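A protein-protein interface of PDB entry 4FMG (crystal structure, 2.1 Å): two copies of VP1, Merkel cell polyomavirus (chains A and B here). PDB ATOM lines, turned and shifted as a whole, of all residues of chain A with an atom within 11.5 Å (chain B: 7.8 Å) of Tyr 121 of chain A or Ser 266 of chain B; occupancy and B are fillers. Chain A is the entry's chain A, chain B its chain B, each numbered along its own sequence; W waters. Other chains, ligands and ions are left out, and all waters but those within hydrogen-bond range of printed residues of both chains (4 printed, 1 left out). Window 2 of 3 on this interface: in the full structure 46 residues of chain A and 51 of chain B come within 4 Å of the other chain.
OE1 of Gln 53 of chain B sits at hydrogen-bond distance from NH1 of Arg 117 of chain A, 2.9 Å away. O of Pro 54 of chain B lies within hydrogen-bond range of NH2 of Arg 117 of chain A, at 3.2 Å. A ring nitrogen (NE2) of His 119 of chain A sits at hydrogen-bond distance from the backbone carbonyl oxygen (O) of Gly 267 of chain B, at 2.9 Å. The backbone NH (N) of Gly 122 of chain A sits close to the backbone carbonyl oxygen (O) of Gly 267 of chain B. The backbone NH (N) of Ala 123 of chain A lies close to the backbone carbonyl oxygen (O) of Leu 52 of chain B (3.5 Å). The backbone NH (N) of Ala 123 of chain A sits at hydrogen-bond distance from the side-chain sulfur (SD) of Met 269 of chain B, at 3.4 Å.
The backbone carbonyl oxygen (O) of Val 110 of chain A sits at hydrogen-bond distance from the backbone NH (N) of Gly 124 of chain A, 2.9 Å away. O of Gly 122 of chain A sits at hydrogen-bond distance from NH1 of Arg 117 of chain A, 3.2 Å away. The backbone NH of Val 118 of chain A is in hydrogen-bond range of the backbone carbonyl oxygen of Ala 123 of chain A (3.0 Å). O of Met 269 of chain B is in hydrogen-bond range of N of Leu 52 of chain B, at 2.8 Å. O of Phe 263 of chain B sits at hydrogen-bond distance from N of Lys 116 of chain B. The backbone NH (N) of Lys 268 of chain B sits at hydrogen-bond distance from the side-chain hydroxyl (OG) of Ser 266 of chain B, 3.3 Å away.
Among the printed residues, merely in contact across the chains: Met 115 of chain A with Pro 54 of chain B, Tyr 121 of chain A with Lys 268 of chain B, Asp 120 of chain A with Gly 267 of chain B, Tyr 121 of chain A with Ser 266 of chain B, Tyr 121 of chain A with Gly 267 of chain B, Val 118 of chain A with Met 269 of chain B, Gly 122 of chain A with Leu 52 of chain B, Gly 122 of chain A with Pro 54 of chain B, Tyr 121 of chain A with Gln 53 of chain B, His 111 of chain A with Gln 53 of chain B, Gly 122 of chain A with Met 269 of chain B, His 119 of chain A with Met 269 of chain B, Gly 124 of chain A with Pro 54 of chain B, His 119 of chain A with Phe 263 of chain B, Asp 120 of chain A with Ser 266 of chain B and His 111 of chain A with Leu 52 of chain B.
Tyr 121 of chain A touches just these residues of chain B: Gln 53, Ser 266, Gly 267 and Lys 268. Printed residues of chain A within 4 Å of Ser 266 of chain B: Asp 120 and Tyr 121. Gly 122 of chain A touches just these residues of chain B: Leu 52, Pro 54, Gly 267 and Met 269. Of chain A, only His 119, Asp 120, Tyr 121 and Gly 122 come within 4 Å of Gly 267 of chain B. Of the printed residues of chain A, Lys 268 of chain B touches Tyr 121. Printed residues of chain A within 4 Å of Gln 53 of chain B: His 111 (3.8 Å), Arg 117 (2.9 Å) and Tyr 121 (3.7 Å). Of the printed residues of chain B, Val 118 of chain A touches Met 269. Of the printed residues of chain B, Asp 120 of chain A touches Ser 266 and Gly 267. Printed residues of chain B within 4 Å of Ala 123 of chain A: Leu 52 and Met 269. Asp 51 of chain B touches none of the printed residues of chain A. Asp 114 of chain B touches none of the printed residues of chain A. The nearest residue of chain B that does not touch Tyr 121 of chain A is Met 269 of chain B (4.5 Å). The nearest residue of chain A that does not touch Ser 266 of chain B is His 119 of chain A (5.8 Å). The nearest printed residue of chain A that does not touch Phe 263 of chain B is Val 118 of chain A (4.9 Å).
Hydrophobic or aromatic side chains of chain A that line the printed part of chain B: His 111, Val 118, His 119, Tyr 121 and Ala 123. Printed residues of chain B that touch a printed residue of chain A: Leu 52, Gln 53, Pro 54, Phe 263, Ser 266, Gly 267, Lys 268 and Met 269. Hydrophobic or aromatic side chains of chain B within 4 Å of the printed part of chain A: Leu 52, Pro 54, Phe 263 and Met 269. Among the printed residues, 22 pairs touch across the chains. Among the printed residues, no Asp or Glu carboxylate lies within 4 Å of a Lys or Arg side-chain nitrogen of the other chain.
Positions printed for both chains: 115, 116 and 265.
Water W2 bridges the backbone carbonyl oxygen of Pro 54 of chain B (2.7 Å) and the guanidinium group of Arg 117 of chain A (3.0 Å). Water W1 lies within hydrogen-bond range of the backbone carbonyl oxygen of Leu 52 of chain B, the backbone NH of Met 269 of chain B and the backbone carbonyl oxygen of Tyr 121 of chain A. Water W3 lies within hydrogen-bond range of O of Asp 120 of chain A and O of Ser 266 of chain B. Water W4 bridges the guanidinium group (NH2) of Arg 117 of chain A and the backbone carbonyl oxygen (O) of Pro 54 of chain B.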
ATOM      1  N   VAL A 110      11.534  10.132 -19.973  1.00  0.00           N
ATOM      2  CA  VAL A 110      10.613   9.483 -20.912  1.00  0.00           C
ATOM      3  C   VAL A 110       9.156   9.740 -20.514  1.00  0.00           C
ATOM      4  O   VAL A 110       8.275   8.900 -20.738  1.00  0.00           O
ATOM      5  CB  VAL A 110      10.889   7.961 -21.046  1.00  0.00           C
ATOM      6  CG1 VAL A 110      12.235   7.715 -21.731  1.00  0.00           C
ATOM      7  CG2 VAL A 110      10.837   7.269 -19.694  1.00  0.00           C
ATOM      8  N   HIS A 111       8.915  10.909 -19.917  1.00  0.00           N
ATOM      9  CA  HIS A 111       7.581  11.301 -19.465  1.00  0.00           C
ATOM     10  C   HIS A 111       7.282  12.776 -19.738  1.00  0.00           C
ATOM     11  O   HIS A 111       6.581  13.429 -18.966  1.00  0.00           O
ATOM     12  CB  HIS A 111       7.397  10.978 -17.976  1.00  0.00           C
ATOM     13  CG  HIS A 111       8.466  11.556 -17.105  1.00  0.00           C
ATOM     14  ND1 HIS A 111       8.394  12.832 -16.586  1.00  0.00           N
ATOM     15  CD2 HIS A 111       9.651  11.047 -16.693  1.00  0.00           C
ATOM     16  CE1 HIS A 111       9.483  13.077 -15.878  1.00  0.00           C
ATOM     17  NE2 HIS A 111      10.263  12.011 -15.931  1.00  0.00           N
ATOM     18  N   MET A 115       4.614  13.245 -25.065  1.00  0.00           N
ATOM     19  CA  MET A 115       5.555  12.344 -25.737  1.00  0.00           C
ATOM     20  C   MET A 115       4.800  11.177 -26.367  1.00  0.00           C
ATOM     21  O   MET A 115       3.934  10.566 -25.736  1.00  0.00           O
ATOM     22  CB  MET A 115       6.585  11.815 -24.732  1.00  0.00           C
ATOM     23  CG  MET A 115       8.049  11.814 -25.182  1.00  0.00           C
ATOM     24  SD  MET A 115       9.137  11.420 -23.775  1.00  0.00           S
ATOM     25  CE  MET A 115      10.723  11.988 -24.366  1.00  0.00           C
ATOM     26  N   LYS A 116       5.131  10.867 -27.615  1.00  0.00           N
ATOM     27  CA  LYS A 116       4.637   9.658 -28.258  1.00  0.00           C
ATOM     28  C   LYS A 116       5.097   8.448 -27.446  1.00  0.00           C
ATOM     29  O   LYS A 116       6.251   8.377 -27.037  1.00  0.00           O
ATOM     30  CB  LYS A 116       5.155   9.579 -29.688  1.00  0.00           C
ATOM     31  CG  LYS A 116       4.665   8.378 -30.472  1.00  0.00           C
ATOM     32  CD  LYS A 116       4.870   8.594 -31.959  1.00  0.00           C
ATOM     33  CE  LYS A 116       4.601   7.318 -32.766  1.00  0.00           C
ATOM     34  NZ  LYS A 116       3.158   6.957 -32.799  1.00  0.00           N
ATOM     35  N   ARG A 117       4.188   7.519 -27.186  1.00  0.00           N
ATOM     36  CA  ARG A 117       4.532   6.322 -26.427  1.00  0.00           C
ATOM     37  C   ARG A 117       5.148   5.269 -27.339  1.00  0.00           C
ATOM     38  O   ARG A 117       4.926   5.293 -28.556  1.00  0.00           O
ATOM     39  CB  ARG A 117       3.297   5.739 -25.759  1.00  0.00           C
ATOM     40  CG  ARG A 117       2.627   6.651 -24.755  1.00  0.00           C
ATOM     41  CD  ARG A 117       1.372   5.978 -24.248  1.00  0.00           C
ATOM     42  NE  ARG A 117       0.545   6.859 -23.433  1.00  0.00           N
ATOM     43  CZ  ARG A 117       0.340   6.706 -22.127  1.00  0.00           C
ATOM     44  NH1 ARG A 117       0.903   5.704 -21.462  1.00  0.00           N
ATOM     45  NH2 ARG A 117      -0.439   7.563 -21.490  1.00  0.00           N
ATOM     46  N   VAL A 118       5.913   4.347 -26.753  1.00  0.00           N
ATOM     47  CA  VAL A 118       6.520   3.263 -27.531  1.00  0.00           C
ATOM     48  C   VAL A 118       5.479   2.198 -27.908  1.00  0.00           C
ATOM     49  O   VAL A 118       5.630   1.498 -28.913  1.00  0.00           O
ATOM     50  CB  VAL A 118       7.762   2.631 -26.824  1.00  0.00           C
ATOM     51  CG1 VAL A 118       8.707   3.719 -26.316  1.00  0.00           C
ATOM     52  CG2 VAL A 118       7.352   1.708 -25.695  1.00  0.00           C
ATOM     53  N   HIS A 119       4.438   2.088 -27.081  1.00  0.00           N
ATOM     54  CA  HIS A 119       3.276   1.225 -27.328  1.00  0.00           C
ATOM     55  C   HIS A 119       2.215   1.628 -26.309  1.00  0.00           C
ATOM     56  O   HIS A 119       2.475   2.461 -25.436  1.00  0.00           O
ATOM     57  CB  HIS A 119       3.606  -0.282 -27.246  1.00  0.00           C
ATOM     58  CG  HIS A 119       4.330  -0.697 -25.998  1.00  0.00           C
ATOM     59  ND1 HIS A 119       5.563  -1.317 -26.026  1.00  0.00           N
ATOM     60  CD2 HIS A 119       3.988  -0.602 -24.689  1.00  0.00           C
ATOM     61  CE1 HIS A 119       5.947  -1.587 -24.791  1.00  0.00           C
ATOM     62  NE2 HIS A 119       5.014  -1.154 -23.960  1.00  0.00           N
ATOM     63  N   ASP A 120       1.020   1.056 -26.409  1.00  0.00           N
ATOM     64  CA  ASP A 120      -0.047   1.412 -25.477  1.00  0.00           C
ATOM     65  C   ASP A 120       0.383   1.250 -24.030  1.00  0.00           C
ATOM     66  O   ASP A 120       0.978   0.231 -23.662  1.00  0.00           O
ATOM     67  CB  ASP A 120      -1.307   0.592 -25.746  1.00  0.00           C
ATOM     68  CG  ASP A 120      -1.958   0.953 -27.056  1.00  0.00           C
ATOM     69  OD1 ASP A 120      -1.768   2.102 -27.508  1.00  0.00           O
ATOM     70  OD2 ASP A 120      -2.656   0.091 -27.632  1.00  0.00           O
ATOM     71  N   TYR A 121       0.092   2.283 -23.235  1.00  0.00           N
ATOM     72  CA  TYR A 121       0.349   2.315 -21.790  1.00  0.00           C
ATOM     73  C   TYR A 121       1.831   2.419 -21.397  1.00  0.00           C
ATOM     74  O   TYR A 121       2.162   2.398 -20.209  1.00  0.00           O
ATOM     75  CB  TYR A 121      -0.334   1.132 -21.078  1.00  0.00           C
ATOM     76  CG  TYR A 121      -1.831   1.078 -21.317  1.00  0.00           C
ATOM     77  CD1 TYR A 121      -2.382   0.148 -22.199  1.00  0.00           C
ATOM     78  CD2 TYR A 121      -2.692   1.979 -20.679  1.00  0.00           C
ATOM     79  CE1 TYR A 121      -3.759   0.107 -22.430  1.00  0.00           C
ATOM     80  CE2 TYR A 121      -4.063   1.948 -20.902  1.00  0.00           C
ATOM     81  CZ  TYR A 121      -4.587   1.014 -21.774  1.00  0.00           C
ATOM     82  OH  TYR A 121      -5.939   0.983 -21.996  1.00  0.00           O
ATOM     83  N   GLY A 122       2.713   2.549 -22.381  1.00  0.00           N
ATOM     84  CA  GLY A 122       4.153   2.556 -22.126  1.00  0.00           C
ATOM     85  C   GLY A 122       4.744   3.930 -21.921  1.00  0.00           C
ATOM     86  O   GLY A 122       4.025   4.924 -21.858  1.00  0.00           O
ATOM     87  N   ALA A 123       6.070   3.974 -21.813  1.00  0.00           N
ATOM     88  CA  ALA A 123       6.803   5.213 -21.631  1.00  0.00           C
ATOM     89  C   ALA A 123       6.922   5.941 -22.955  1.00  0.00           C
ATOM     90  O   ALA A 123       6.711   5.356 -24.017  1.00  0.00           O
ATOM     91  CB  ALA A 123       8.185   4.925 -21.053  1.00  0.00           C
ATOM     92  N   GLY A 124       7.251   7.228 -22.890  1.00  0.00           N
ATOM     93  CA  GLY A 124       7.530   7.998 -24.086  1.00  0.00           C
ATOM     94  C   GLY A 124       8.762   7.457 -24.785  1.00  0.00           C
ATOM     95  O   GLY A 124       9.649   6.893 -24.131  1.00  0.00           O
ATOM     96  N   ILE A 125       8.788   7.586 -26.114  1.00  0.00           N
ATOM     97  CA  ILE A 125       9.990   7.315 -26.910  1.00  0.00           C
ATOM     98  C   ILE A 125      11.031   8.356 -26.505  1.00  0.00           C
ATOM     99  O   ILE A 125      10.779   9.566 -26.637  1.00  0.00           O
ATOM    100  CB  ILE A 125       9.727   7.416 -28.432  1.00  0.00           C
ATOM    101  CG1 ILE A 125       8.612   6.449 -28.860  1.00  0.00           C
ATOM    102  CG2 ILE A 125      11.024   7.159 -29.239  1.00  0.00           C
ATOM    103  CD1 ILE A 125       8.085   6.682 -30.265  1.00  0.00           C
ATOM    104  N   THR A 265       3.069  13.218 -29.386  1.00  0.00           N
ATOM    105  CA  THR A 265       1.937  12.284 -29.462  1.00  0.00           C
ATOM    106  C   THR A 265       1.298  12.222 -30.853  1.00  0.00           C
ATOM    107  O   THR A 265       0.948  11.133 -31.338  1.00  0.00           O
ATOM    108  CB  THR A 265       0.845  12.641 -28.417  1.00  0.00           C
ATOM    109  OG1 THR A 265       1.437  12.746 -27.118  1.00  0.00           O
ATOM    110  CG2 THR A 265      -0.251  11.581 -28.381  1.00  0.00           C
ATOM    111  N   ASP B  51       5.371   3.248 -12.732  1.00  0.00           N
ATOM    112  CA  ASP B  51       5.157   3.204 -14.174  1.00  0.00           C
ATOM    113  C   ASP B  51       5.362   4.580 -14.822  1.00  0.00           C
ATOM    114  O   ASP B  51       4.794   5.581 -14.388  1.00  0.00           O
ATOM    115  CB  ASP B  51       3.783   2.595 -14.480  1.00  0.00           C
ATOM    116  CG  ASP B  51       3.663   1.145 -13.989  1.00  0.00           C
ATOM    117  OD1 ASP B  51       2.601   0.774 -13.457  1.00  0.00           O
ATOM    118  OD2 ASP B  51       4.635   0.370 -14.116  1.00  0.00           O
ATOM    119  N   LEU B  52       6.201   4.626 -15.847  1.00  0.00           N
ATOM    120  CA  LEU B  52       6.507   5.880 -16.531  1.00  0.00           C
ATOM    121  C   LEU B  52       5.588   6.085 -17.729  1.00  0.00           C
ATOM    122  O   LEU B  52       5.545   5.265 -18.635  1.00  0.00           O
ATOM    123  CB  LEU B  52       7.982   5.924 -16.945  1.00  0.00           C
ATOM    124  CG  LEU B  52       8.968   5.958 -15.769  1.00  0.00           C
ATOM    125  CD1 LEU B  52      10.287   5.300 -16.134  1.00  0.00           C
ATOM    126  CD2 LEU B  52       9.204   7.375 -15.288  1.00  0.00           C
ATOM    127  N   GLN B  53       4.847   7.185 -17.717  1.00  0.00           N
ATOM    128  CA  GLN B  53       3.849   7.471 -18.746  1.00  0.00           C
ATOM    129  C   GLN B  53       3.792   8.959 -19.081  1.00  0.00           C
ATOM    130  O   GLN B  53       3.835   9.786 -18.179  1.00  0.00           O
ATOM    131  CB  GLN B  53       2.460   7.054 -18.256  1.00  0.00           C
ATOM    132  CG  GLN B  53       2.201   5.563 -18.163  1.00  0.00           C
ATOM    133  CD  GLN B  53       0.738   5.266 -17.902  1.00  0.00           C
ATOM    134  OE1 GLN B  53      -0.042   5.077 -18.834  1.00  0.00           O
ATOM    135  NE2 GLN B  53       0.351   5.259 -16.632  1.00  0.00           N
ATOM    136  N   PRO B  54       3.677   9.307 -20.376  1.00  0.00           N
ATOM    137  CA  PRO B  54       3.277  10.678 -20.697  1.00  0.00           C
ATOM    138  C   PRO B  54       1.889  10.945 -20.110  1.00  0.00           C
ATOM    139  O   PRO B  54       1.012  10.077 -20.177  1.00  0.00           O
ATOM    140  CB  PRO B  54       3.192  10.685 -22.222  1.00  0.00           C
ATOM    141  CG  PRO B  54       3.962   9.504 -22.673  1.00  0.00           C
ATOM    142  CD  PRO B  54       3.901   8.491 -21.582  1.00  0.00           C
ATOM    143  N   ASP B 114       4.968 -11.049 -14.668  1.00  0.00           N
ATOM    144  CA  ASP B 114       4.130 -10.085 -15.385  1.00  0.00           C
ATOM    145  C   ASP B 114       4.917  -9.370 -16.491  1.00  0.00           C
ATOM    146  O   ASP B 114       4.654  -8.205 -16.811  1.00  0.00           O
ATOM    147  CB  ASP B 114       3.527  -9.075 -14.400  1.00  0.00           C
ATOM    148  CG  ASP B 114       2.332  -8.328 -14.970  1.00  0.00           C
ATOM    149  OD1 ASP B 114       1.589  -8.904 -15.784  1.00  0.00           O
ATOM    150  OD2 ASP B 114       2.128  -7.157 -14.589  1.00  0.00           O
ATOM    151  N   MET B 115       5.871 -10.085 -17.078  1.00  0.00           N
ATOM    152  CA  MET B 115       6.703  -9.537 -18.142  1.00  0.00           C
ATOM    153  C   MET B 115       5.951  -9.572 -19.465  1.00  0.00           C
ATOM    154  O   MET B 115       5.349 -10.585 -19.809  1.00  0.00           O
ATOM    155  CB  MET B 115       7.985 -10.360 -18.272  1.00  0.00           C
ATOM    156  CG  MET B 115       9.236  -9.560 -18.560  1.00  0.00           C
ATOM    157  SD  MET B 115      10.696 -10.590 -18.315  1.00  0.00           S
ATOM    158  CE  MET B 115      11.942  -9.340 -17.952  1.00  0.00           C
ATOM    159  N   LYS B 116       6.003  -8.473 -20.213  1.00  0.00           N
ATOM    160  CA  LYS B 116       5.485  -8.443 -21.580  1.00  0.00           C
ATOM    161  C   LYS B 116       6.325  -9.358 -22.471  1.00  0.00           C
ATOM    162  O   LYS B 116       7.552  -9.311 -22.434  1.00  0.00           O
ATOM    163  CB  LYS B 116       5.491  -7.007 -22.120  1.00  0.00           C
ATOM    164  CG  LYS B 116       4.972  -6.862 -23.547  1.00  0.00           C
ATOM    165  CD  LYS B 116       4.763  -5.390 -23.940  1.00  0.00           C
ATOM    166  CE  LYS B 116       4.336  -5.248 -25.401  1.00  0.00           C
ATOM    167  NZ  LYS B 116       3.053  -5.949 -25.635  1.00  0.00           N
ATOM    168  N   PHE B 263       9.548  -4.317 -18.758  1.00  0.00           N
ATOM    169  CA  PHE B 263       8.354  -4.248 -19.605  1.00  0.00           C
ATOM    170  C   PHE B 263       7.265  -5.142 -19.036  1.00  0.00           C
ATOM    171  O   PHE B 263       7.417  -6.368 -18.990  1.00  0.00           O
ATOM    172  CB  PHE B 263       8.677  -4.704 -21.029  1.00  0.00           C
ATOM    173  CG  PHE B 263       9.495  -3.724 -21.817  1.00  0.00           C
ATOM    174  CD1 PHE B 263      10.884  -3.707 -21.708  1.00  0.00           C
ATOM    175  CD2 PHE B 263       8.880  -2.829 -22.682  1.00  0.00           C
ATOM    176  CE1 PHE B 263      11.648  -2.803 -22.439  1.00  0.00           C
ATOM    177  CE2 PHE B 263       9.637  -1.921 -23.420  1.00  0.00           C
ATOM    178  CZ  PHE B 263      11.023  -1.909 -23.296  1.00  0.00           C
ATOM    179  N   LYS B 264       6.159  -4.521 -18.630  1.00  0.00           N
ATOM    180  CA  LYS B 264       5.053  -5.233 -18.003  1.00  0.00           C
ATOM    181  C   LYS B 264       3.967  -5.609 -19.022  1.00  0.00           C
ATOM    182  O   LYS B 264       3.790  -4.917 -20.030  1.00  0.00           O
ATOM    183  CB  LYS B 264       4.472  -4.402 -16.848  1.00  0.00           C
ATOM    184  CG  LYS B 264       5.487  -4.081 -15.762  1.00  0.00           C
ATOM    185  CD  LYS B 264       4.944  -3.117 -14.743  1.00  0.00           C
ATOM    186  CE  LYS B 264       5.988  -2.804 -13.659  1.00  0.00           C
ATOM    187  NZ  LYS B 264       5.480  -1.751 -12.731  1.00  0.00           N
ATOM    188  N   THR B 265       3.261  -6.707 -18.741  1.00  0.00           N
ATOM    189  CA  THR B 265       2.231  -7.278 -19.625  1.00  0.00           C
ATOM    190  C   THR B 265       1.251  -6.252 -20.209  1.00  0.00           C
ATOM    191  O   THR B 265       0.937  -6.296 -21.398  1.00  0.00           O
ATOM    192  CB  THR B 265       1.433  -8.379 -18.882  1.00  0.00           C
ATOM    193  OG1 THR B 265       2.351  -9.340 -18.347  1.00  0.00           O
ATOM    194  CG2 THR B 265       0.439  -9.091 -19.812  1.00  0.00           C
ATOM    195  N   SER B 266       0.790  -5.333 -19.362  1.00  0.00           N
ATOM    196  CA  SER B 266      -0.145  -4.271 -19.745  1.00  0.00           C
ATOM    197  C   SER B 266       0.417  -3.302 -20.779  1.00  0.00           C
ATOM    198  O   SER B 266      -0.338  -2.633 -21.482  1.00  0.00           O
ATOM    199  CB  SER B 266      -0.536  -3.474 -18.503  1.00  0.00           C
ATOM    200  OG  SER B 266       0.628  -2.942 -17.871  1.00  0.00           O
ATOM    201  N   GLY B 267       1.738  -3.210 -20.853  1.00  0.00           N
ATOM    202  CA  GLY B 267       2.385  -2.223 -21.708  1.00  0.00           C
ATOM    203  C   GLY B 267       3.115  -1.189 -20.877  1.00  0.00           C
ATOM    204  O   GLY B 267       3.927  -0.425 -21.397  1.00  0.00           O
ATOM    205  N   LYS B 268       2.834  -1.175 -19.575  1.00  0.00           N
ATOM    206  CA  LYS B 268       3.486  -0.249 -18.654  1.00  0.00           C
ATOM    207  C   LYS B 268       4.981  -0.551 -18.474  1.00  0.00           C
ATOM    208  O   LYS B 268       5.417  -1.708 -18.595  1.00  0.00           O
ATOM    209  CB  LYS B 268       2.732  -0.190 -17.325  1.00  0.00           C
ATOM    210  CG  LYS B 268       1.429   0.577 -17.474  1.00  0.00           C
ATOM    211  CD  LYS B 268       0.552   0.531 -16.263  1.00  0.00           C
ATOM    212  CE  LYS B 268      -0.741   1.307 -16.539  1.00  0.00           C
ATOM    213  NZ  LYS B 268      -1.520   1.523 -15.302  1.00  0.00           N
ATOM    214  N   MET B 269       5.758   0.502 -18.227  1.00  0.00           N
ATOM    215  CA  MET B 269       7.217   0.394 -18.169  1.00  0.00           C
ATOM    216  C   MET B 269       7.800   1.148 -16.978  1.00  0.00           C
ATOM    217  O   MET B 269       7.443   2.298 -16.709  1.00  0.00           O
ATOM    218  CB  MET B 269       7.845   0.909 -19.467  1.00  0.00           C
ATOM    219  CG  MET B 269       7.578   0.035 -20.692  1.00  0.00           C
ATOM    220  SD  MET B 269       7.603   1.009 -22.202  1.00  0.00           S
ATOM    221  CE  MET B 269       9.334   1.498 -22.306  1.00  0.00           C
HETATM  222  O   HOH W   1       4.291   2.883 -18.277  1.00  0.00           O
HETATM  223  O   HOH W   2      -0.800   8.776 -18.740  1.00  0.00           O
HETATM  224  O   HOH W   3       0.720  -2.460 -24.741  1.00  0.00           O
HETATM  225  O   HOH W   4      -0.320  10.297 -23.039  1.00  0.00           O
